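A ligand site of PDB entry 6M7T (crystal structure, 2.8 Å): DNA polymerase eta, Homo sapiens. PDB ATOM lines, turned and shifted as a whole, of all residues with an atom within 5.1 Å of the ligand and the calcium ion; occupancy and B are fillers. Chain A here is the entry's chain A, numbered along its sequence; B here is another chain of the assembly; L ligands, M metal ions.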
ATOM      1  N   ASP A  16      -3.135  28.315  19.460  1.00  0.00           N
ATOM      2  CA  ASP A  16      -2.233  27.978  20.550  1.00  0.00           C
ATOM      3  C   ASP A  16      -2.150  29.160  21.503  1.00  0.00           C
ATOM      4  O   ASP A  16      -1.855  30.290  21.080  1.00  0.00           O
ATOM      5  CB  ASP A  16      -0.842  27.719  19.959  1.00  0.00           C
ATOM      6  CG  ASP A  16       0.221  27.431  20.995  1.00  0.00           C
ATOM      7  OD1 ASP A  16      -0.116  27.274  22.177  1.00  0.00           O
ATOM      8  OD2 ASP A  16       1.413  27.369  20.621  1.00  0.00           O
ATOM      9  N   MET A  17      -2.392  28.900  22.783  1.00  0.00           N
ATOM     10  CA  MET A  17      -2.315  29.931  23.804  1.00  0.00           C
ATOM     11  C   MET A  17      -0.890  30.392  24.052  1.00  0.00           C
ATOM     12  O   MET A  17       0.038  29.572  24.077  1.00  0.00           O
ATOM     13  CB  MET A  17      -2.909  29.435  25.105  1.00  0.00           C
ATOM     14  CG  MET A  17      -4.266  28.865  24.909  1.00  0.00           C
ATOM     15  SD  MET A  17      -5.443  30.139  24.467  1.00  0.00           S
ATOM     16  CE  MET A  17      -6.794  29.052  24.198  1.00  0.00           C
ATOM     17  N   ASP A  18      -0.702  31.694  24.209  1.00  0.00           N
ATOM     18  CA  ASP A  18       0.611  32.239  24.545  1.00  0.00           C
ATOM     19  C   ASP A  18       0.836  32.040  26.027  1.00  0.00           C
ATOM     20  O   ASP A  18      -0.066  32.341  26.818  1.00  0.00           O
ATOM     21  CB  ASP A  18       0.719  33.689  24.104  1.00  0.00           C
ATOM     22  CG  ASP A  18       0.543  33.831  22.622  1.00  0.00           C
ATOM     23  OD1 ASP A  18       1.077  32.959  21.877  1.00  0.00           O
ATOM     24  OD2 ASP A  18      -0.148  34.776  22.195  1.00  0.00           O
ATOM     25  N   CYS A  19       2.023  31.546  26.410  1.00  0.00           N
ATOM     26  CA  CYS A  19       2.400  31.282  27.806  1.00  0.00           C
ATOM     27  C   CYS A  19       1.160  30.994  28.658  1.00  0.00           C
ATOM     28  O   CYS A  19       0.814  31.733  29.580  1.00  0.00           O
ATOM     29  CB  CYS A  19       3.206  32.454  28.376  1.00  0.00           C
ATOM     30  SG  CYS A  19       2.436  34.149  28.262  1.00  0.00           S
ATOM     31  N   PHE A  20       0.480  29.916  28.283  1.00  0.00           N
ATOM     32  CA  PHE A  20      -0.784  29.510  28.895  1.00  0.00           C
ATOM     33  C   PHE A  20      -0.771  29.557  30.424  1.00  0.00           C
ATOM     34  O   PHE A  20      -1.591  30.244  31.037  1.00  0.00           O
ATOM     35  CB  PHE A  20      -1.159  28.111  28.410  1.00  0.00           C
ATOM     36  CG  PHE A  20      -2.542  27.678  28.816  1.00  0.00           C
ATOM     37  CD1 PHE A  20      -3.639  28.502  28.565  1.00  0.00           C
ATOM     38  CD2 PHE A  20      -2.756  26.431  29.384  1.00  0.00           C
ATOM     39  CE1 PHE A  20      -4.923  28.094  28.923  1.00  0.00           C
ATOM     40  CE2 PHE A  20      -4.040  26.023  29.741  1.00  0.00           C
ATOM     41  CZ  PHE A  20      -5.134  26.860  29.508  1.00  0.00           C
ATOM     42  N   PHE A  21       0.148  28.812  31.055  1.00  0.00           N
ATOM     43  CA  PHE A  21       0.203  28.785  32.513  1.00  0.00           C
ATOM     44  C   PHE A  21       0.409  30.181  33.092  1.00  0.00           C
ATOM     45  O   PHE A  21      -0.186  30.554  34.118  1.00  0.00           O
ATOM     46  CB  PHE A  21       1.305  27.835  32.981  1.00  0.00           C
ATOM     47  CG  PHE A  21       0.927  26.379  32.900  1.00  0.00           C
ATOM     48  CD1 PHE A  21      -0.145  25.963  32.120  1.00  0.00           C
ATOM     49  CD2 PHE A  21       1.642  25.419  33.609  1.00  0.00           C
ATOM     50  CE1 PHE A  21      -0.498  24.619  32.025  1.00  0.00           C
ATOM     51  CE2 PHE A  21       1.297  24.068  33.523  1.00  0.00           C
ATOM     52  CZ  PHE A  21       0.226  23.682  32.732  1.00  0.00           C
ATOM     53  N   VAL A  22       1.250  30.991  32.443  1.00  0.00           N
ATOM     54  CA  VAL A  22       1.469  32.332  32.937  1.00  0.00           C
ATOM     55  C   VAL A  22       0.159  33.108  32.896  1.00  0.00           C
ATOM     56  O   VAL A  22      -0.229  33.728  33.886  1.00  0.00           O
ATOM     57  CB  VAL A  22       2.563  33.047  32.132  1.00  0.00           C
ATOM     58  CG1 VAL A  22       2.582  34.526  32.452  1.00  0.00           C
ATOM     59  CG2 VAL A  22       3.913  32.427  32.416  1.00  0.00           C
ATOM     60  N   ILE A  51       8.684  26.642  34.375  1.00  0.00           N
ATOM     61  CA  ILE A  51       7.952  25.930  33.343  1.00  0.00           C
ATOM     62  C   ILE A  51       7.227  26.866  32.388  1.00  0.00           C
ATOM     63  O   ILE A  51       6.997  26.492  31.232  1.00  0.00           O
ATOM     64  CB  ILE A  51       6.949  24.915  33.943  1.00  0.00           C
ATOM     65  CG1 ILE A  51       6.105  25.525  35.062  1.00  0.00           C
ATOM     66  CG2 ILE A  51       7.691  23.740  34.543  1.00  0.00           C
ATOM     67  CD1 ILE A  51       5.128  24.528  35.673  1.00  0.00           C
ATOM     68  N   ALA A  52       6.810  28.052  32.837  1.00  0.00           N
ATOM     69  CA  ALA A  52       6.106  28.967  31.923  1.00  0.00           C
ATOM     70  C   ALA A  52       6.659  30.378  32.062  1.00  0.00           C
ATOM     71  O   ALA A  52       6.729  30.906  33.171  1.00  0.00           O
ATOM     72  CB  ALA A  52       4.596  28.958  32.193  1.00  0.00           C
ATOM     73  N   VAL A  53       7.073  30.983  30.949  1.00  0.00           N
ATOM     74  CA  VAL A  53       7.667  32.315  30.993  1.00  0.00           C
ATOM     75  C   VAL A  53       6.853  33.286  30.164  1.00  0.00           C
ATOM     76  O   VAL A  53       6.470  32.988  29.029  1.00  0.00           O
ATOM     77  CB  VAL A  53       9.109  32.275  30.433  1.00  0.00           C
ATOM     78  CG1 VAL A  53       9.769  33.645  30.555  1.00  0.00           C
ATOM     79  CG2 VAL A  53       9.923  31.177  31.080  1.00  0.00           C
ATOM     80  N   TYR A  55       6.066  36.694  27.965  1.00  0.00           N
ATOM     81  CA  TYR A  55       6.839  37.296  26.885  1.00  0.00           C
ATOM     82  C   TYR A  55       7.654  38.481  27.392  1.00  0.00           C
ATOM     83  O   TYR A  55       8.775  38.698  26.920  1.00  0.00           O
ATOM     84  CB  TYR A  55       5.944  37.685  25.699  1.00  0.00           C
ATOM     85  CG  TYR A  55       5.640  36.504  24.802  1.00  0.00           C
ATOM     86  CD1 TYR A  55       6.459  36.217  23.717  1.00  0.00           C
ATOM     87  CD2 TYR A  55       4.534  35.689  25.014  1.00  0.00           C
ATOM     88  CE1 TYR A  55       6.197  35.151  22.880  1.00  0.00           C
ATOM     89  CE2 TYR A  55       4.271  34.615  24.182  1.00  0.00           C
ATOM     90  CZ  TYR A  55       5.104  34.358  23.106  1.00  0.00           C
ATOM     91  OH  TYR A  55       4.874  33.289  22.270  1.00  0.00           O
ATOM     92  N   ARG A  58      10.855  37.172  28.546  1.00  0.00           N
ATOM     93  CA  ARG A  58      11.723  36.570  27.540  1.00  0.00           C
ATOM     94  C   ARG A  58      12.690  37.578  26.957  1.00  0.00           C
ATOM     95  O   ARG A  58      13.763  37.194  26.473  1.00  0.00           O
ATOM     96  CB  ARG A  58      10.878  35.956  26.433  1.00  0.00           C
ATOM     97  CG  ARG A  58      10.020  34.813  26.927  1.00  0.00           C
ATOM     98  CD  ARG A  58       9.235  34.188  25.800  1.00  0.00           C
ATOM     99  NE  ARG A  58       8.239  33.253  26.323  1.00  0.00           N
ATOM    100  CZ  ARG A  58       7.552  32.400  25.579  1.00  0.00           C
ATOM    101  NH1 ARG A  58       7.762  32.350  24.270  1.00  0.00           N
ATOM    102  NH2 ARG A  58       6.664  31.598  26.147  1.00  0.00           N
ATOM    103  N   ARG A  64      12.737  28.607  29.586  1.00  0.00           N
ATOM    104  CA  ARG A  64      12.229  27.531  30.435  1.00  0.00           C
ATOM    105  C   ARG A  64      13.376  26.566  30.743  1.00  0.00           C
ATOM    106  O   ARG A  64      14.431  26.616  30.107  1.00  0.00           O
ATOM    107  CB  ARG A  64      11.136  26.775  29.670  1.00  0.00           C
ATOM    108  CG  ARG A  64      10.641  25.469  30.305  1.00  0.00           C
ATOM    109  CD  ARG A  64       9.586  24.715  29.486  1.00  0.00           C
ATOM    110  NE  ARG A  64       8.285  25.355  29.303  1.00  0.00           N
ATOM    111  CZ  ARG A  64       7.709  25.522  28.122  1.00  0.00           C
ATOM    112  NH1 ARG A  64       6.518  26.096  28.041  1.00  0.00           N
ATOM    113  NH2 ARG A  64       8.322  25.115  27.023  1.00  0.00           N
ATOM    114  N   ILE A 117      -3.491  20.600  25.926  1.00  0.00           N
ATOM    115  CA  ILE A 117      -4.050  21.434  26.979  1.00  0.00           C
ATOM    116  C   ILE A 117      -4.191  22.892  26.550  1.00  0.00           C
ATOM    117  O   ILE A 117      -5.054  23.615  27.087  1.00  0.00           O
ATOM    118  CB  ILE A 117      -3.143  21.313  28.235  1.00  0.00           C
ATOM    119  CG1 ILE A 117      -3.834  21.853  29.491  1.00  0.00           C
ATOM    120  CG2 ILE A 117      -1.757  21.927  27.981  1.00  0.00           C
ATOM    121  CD1 ILE A 117      -4.830  20.886  30.055  1.00  0.00           C
ATOM    122  N   ASP A 118      -3.394  23.353  25.571  1.00  0.00           N
ATOM    123  CA  ASP A 118      -3.464  24.749  25.141  1.00  0.00           C
ATOM    124  C   ASP A 118      -3.572  24.924  23.633  1.00  0.00           C
ATOM    125  O   ASP A 118      -3.325  26.032  23.139  1.00  0.00           O
ATOM    126  CB  ASP A 118      -2.327  25.593  25.714  1.00  0.00           C
ATOM    127  CG  ASP A 118      -1.073  25.528  24.903  1.00  0.00           C
ATOM    128  OD1 ASP A 118      -0.367  26.545  24.874  1.00  0.00           O
ATOM    129  OD2 ASP A 118      -0.767  24.467  24.330  1.00  0.00           O
ATOM    130  N   GLU A 119      -3.970  23.911  22.870  1.00  0.00           N
ATOM    131  CA  GLU A 119      -4.059  24.097  21.429  1.00  0.00           C
ATOM    132  C   GLU A 119      -5.189  23.267  20.861  1.00  0.00           C
ATOM    133  O   GLU A 119      -5.501  22.179  21.351  1.00  0.00           O
ATOM    134  CB  GLU A 119      -2.795  23.574  20.704  1.00  0.00           C
ATOM    135  CG  GLU A 119      -1.446  23.961  21.269  1.00  0.00           C
ATOM    136  CD  GLU A 119      -0.340  23.888  20.237  1.00  0.00           C
ATOM    137  OE1 GLU A 119      -0.516  23.157  19.224  1.00  0.00           O
ATOM    138  OE2 GLU A 119       0.718  24.538  20.445  1.00  0.00           O
ATOM    139  N   LYS A 234       3.953  35.322  16.832  1.00  0.00           N
ATOM    140  CA  LYS A 234       3.476  35.294  18.202  1.00  0.00           C
ATOM    141  C   LYS A 234       4.065  36.507  18.932  1.00  0.00           C
ATOM    142  O   LYS A 234       5.176  36.932  18.611  1.00  0.00           O
ATOM    143  CB  LYS A 234       3.887  34.037  18.962  1.00  0.00           C
ATOM    144  CG  LYS A 234       2.962  32.823  18.857  1.00  0.00           C
ATOM    145  CD  LYS A 234       3.592  31.648  19.601  1.00  0.00           C
ATOM    146  CE  LYS A 234       2.606  30.527  19.900  1.00  0.00           C
ATOM    147  NZ  LYS A 234       1.467  30.944  20.794  1.00  0.00           N
ATOM    148  O5'  DA B   1       7.751  16.614  31.821  1.00  0.00           O
ATOM    149  C5'  DA B   1       9.137  16.725  31.509  1.00  0.00           C
ATOM    150  C4'  DA B   1       9.404  16.534  30.013  1.00  0.00           C
ATOM    151  O4'  DA B   1       8.158  16.398  29.281  1.00  0.00           O
ATOM    152  C3'  DA B   1      10.169  17.678  29.354  1.00  0.00           C
ATOM    153  O3'  DA B   1      11.121  17.187  28.442  1.00  0.00           O
ATOM    154  C2'  DA B   1       9.097  18.503  28.647  1.00  0.00           C
ATOM    155  C1'  DA B   1       7.918  17.552  28.488  1.00  0.00           C
ATOM    156  N9   DA B   1       6.653  18.144  28.908  1.00  0.00           N
ATOM    157  C8   DA B   1       6.210  18.343  30.199  1.00  0.00           C
ATOM    158  N7   DA B   1       5.027  18.918  30.285  1.00  0.00           N
ATOM    159  C5   DA B   1       4.675  19.107  28.962  1.00  0.00           C
ATOM    160  C6   DA B   1       3.528  19.667  28.376  1.00  0.00           C
ATOM    161  N6   DA B   1       2.508  20.130  29.090  1.00  0.00           N
ATOM    162  N1   DA B   1       3.492  19.724  27.010  1.00  0.00           N
ATOM    163  C2   DA B   1       4.534  19.249  26.301  1.00  0.00           C
ATOM    164  N3   DA B   1       5.663  18.677  26.753  1.00  0.00           N
ATOM    165  C4   DA B   1       5.672  18.646  28.099  1.00  0.00           C
ATOM    166  P   02I B   3      12.963  15.499  34.408  1.00  0.00           P
ATOM    167  N1  02I B   3       7.907  20.926  32.655  1.00  0.00           N
ATOM    168  C2  02I B   3       7.011  20.584  33.603  1.00  0.00           C
ATOM    169  N3  02I B   3       7.151  19.701  34.579  1.00  0.00           N
ATOM    170  C4  02I B   3       8.367  19.128  34.519  1.00  0.00           C
ATOM    171  C5  02I B   3       9.385  19.361  33.619  1.00  0.00           C
ATOM    172  C6  02I B   3       9.124  20.329  32.630  1.00  0.00           C
ATOM    173  N6  02I B   3       9.982  20.696  31.659  1.00  0.00           N
ATOM    174  N7  02I B   3      10.491  18.579  33.893  1.00  0.00           N
ATOM    175  C8  02I B   3      10.131  17.879  34.943  1.00  0.00           C
ATOM    176  N9  02I B   3       8.857  18.176  35.359  1.00  0.00           N
ATOM    177  C1' 02I B   3       8.190  17.547  36.507  1.00  0.00           C
ATOM    178  C2' 02I B   3       7.579  16.228  36.130  1.00  0.00           C
ATOM    179  OP2 02I B   3      13.019  14.588  33.206  1.00  0.00           O
ATOM    180  C3' 02I B   3       8.836  15.343  36.020  1.00  0.00           C
ATOM    181  O3' 02I B   3       8.598  14.082  36.631  1.00  0.00           O
ATOM    182  C4' 02I B   3       9.947  16.176  36.673  1.00  0.00           C
ATOM    183  O4' 02I B   3       9.256  17.245  37.378  1.00  0.00           O
ATOM    184  C5' 02I B   3      10.939  16.829  35.685  1.00  0.00           C
ATOM    185  O5' 02I B   3      11.376  15.815  34.771  1.00  0.00           O
ATOM    186  OP1 02I B   3      13.743  14.911  35.561  1.00  0.00           O
HETATM  187  P1  LIG L   1       3.549  25.530  25.345  1.00  0.00           P
HETATM  188  O1  LIG L   1       2.408  25.793  24.393  1.00  0.00           O
HETATM  189  O2  LIG L   1       4.604  24.705  24.647  1.00  0.00           O
HETATM  190  O3  LIG L   1       4.204  26.960  25.840  1.00  0.00           O
HETATM  191  P2  LIG L   1       3.544  28.342  26.447  1.00  0.00           P
HETATM  192  O4  LIG L   1       2.034  28.239  26.398  1.00  0.00           O
HETATM  193  O5  LIG L   1       3.990  28.514  27.877  1.00  0.00           O
HETATM  194  O6  LIG L   1       4.030  29.632  25.560  1.00  0.00           O
HETATM  195  P3  LIG L   1       4.062  29.911  23.983  1.00  0.00           P
HETATM  196  O7  LIG L   1       3.788  31.371  23.728  1.00  0.00           O
HETATM  197  O8  LIG L   1       2.990  29.078  23.305  1.00  0.00           O
HETATM  198  O9  LIG L   1       5.412  29.543  23.425  1.00  0.00           O
HETATM  199  O10 LIG L   1       2.986  24.708  26.658  1.00  0.00           O
HETATM  200  C1  LIG L   1       1.717  25.013  27.152  1.00  0.00           C
HETATM  201  C2  LIG L   1       1.691  24.825  28.683  1.00  0.00           C
HETATM  202  O11 LIG L   1       2.156  23.491  29.023  1.00  0.00           O
HETATM  203  C3  LIG L   1       2.657  25.803  29.346  1.00  0.00           C
HETATM  204  O12 LIG L   1       1.945  26.981  29.826  1.00  0.00           O
HETATM  205  C4  LIG L   1       3.210  25.017  30.512  1.00  0.00           C
HETATM  206  C5  LIG L   1       3.123  23.568  30.069  1.00  0.00           C
HETATM  207  N1  LIG L   1       4.400  23.003  29.604  1.00  0.00           N
HETATM  208  C6  LIG L   1       5.408  22.493  30.556  1.00  0.00           C
HETATM  209  O13 LIG L   1       5.169  22.544  31.728  1.00  0.00           O
HETATM  210  N2  LIG L   1       6.636  21.955  30.198  1.00  0.00           N
HETATM  211  C7  LIG L   1       6.871  21.916  28.876  1.00  0.00           C
HETATM  212  O14 LIG L   1       7.979  21.430  28.479  1.00  0.00           O
HETATM  213  C8  LIG L   1       5.938  22.398  27.802  1.00  0.00           C
HETATM  214  C9  LIG L   1       6.293  22.311  26.325  1.00  0.00           C
HETATM  215  C10 LIG L   1       4.734  22.946  28.244  1.00  0.00           C
HETATM  216 CA    CA M   1       1.243  27.876  24.226  1.00  0.00          CA
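Of the 19 residues printed, 3 come within 4 Å of the calcium ion.
Asp 18 touches the ligand (CA to O7, 3.4 Å). Ile 51 touches the ligand (CB to O13, 3.7 Å). Hydrophobic or aromatic side chains within 4 Å of the ligand: Phe 20, Phe 21, Ile 51 and Tyr 55. Within 4 Å of the ligand: Asp 16, Met 17, Asp 18, Cys 19, Phe 20, Phe 21, Ile 51, Tyr 55, Arg 58, Arg 64, Asp 118, Lys 234, DA 1 of chain B and 02I 3 of chain B. Along chain A the residues within 4 Å of the ligand span positions 16 to 234. The nearest printed residue that does not touch the ligand is Ala 52 (4.1 Å).
The calcium ion is bound by O of Met 17, 2.1 Å away. OD1 of Asp 118 is bound to the calcium ion (2.2 Å). An oxygen (O8) of the ligand binds the calcium ion, 2.3 Å away. O4 of the ligand is bound to the calcium ion (2.3 Å). The calcium ion is bound by an oxygen (O1) of the ligand (2.4 Å). OD1 of Asp 16 is bound to the calcium ion (2.5 Å).
O7 of the ligand is in hydrogen-bond range of OH of Tyr 55. O12 of the ligand is in hydrogen-bond range of N of Phe 21 (2.8 Å). O6 of the ligand sits at hydrogen-bond distance from N of Cys 19 (2.9 Å). N1 of 02I 3 of chain B sits at hydrogen-bond distance from a nitrogen (N2) of the ligand (3.0 Å). N of Phe 20 sits close to O4 of the ligand (3.0 Å). N7 of DA 1 of chain B is in hydrogen-bond range of a nitrogen (N2) of the ligand (3.4 Å). The guanidinium group (NH1) of Arg 64 lies within salt-bridge range of an oxygen (O5) of the ligand, 3.5 Å away. O9 of the ligand lies within salt-bridge range of NH2 of Arg 58, at 3.6 Å. O7 of the ligand lies within salt-bridge range of NZ of Lys 234 (3.8 Å).
OD2 of Asp 16 is in salt-bridge range of NZ of Lys 234. The guanidinium group (NE) of Arg 64 sits at hydrogen-bond distance from the backbone carbonyl oxygen (O) of Ile 51, 2.6 Å away. NH2 of Arg 58 is in hydrogen-bond range of O of Val 53.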
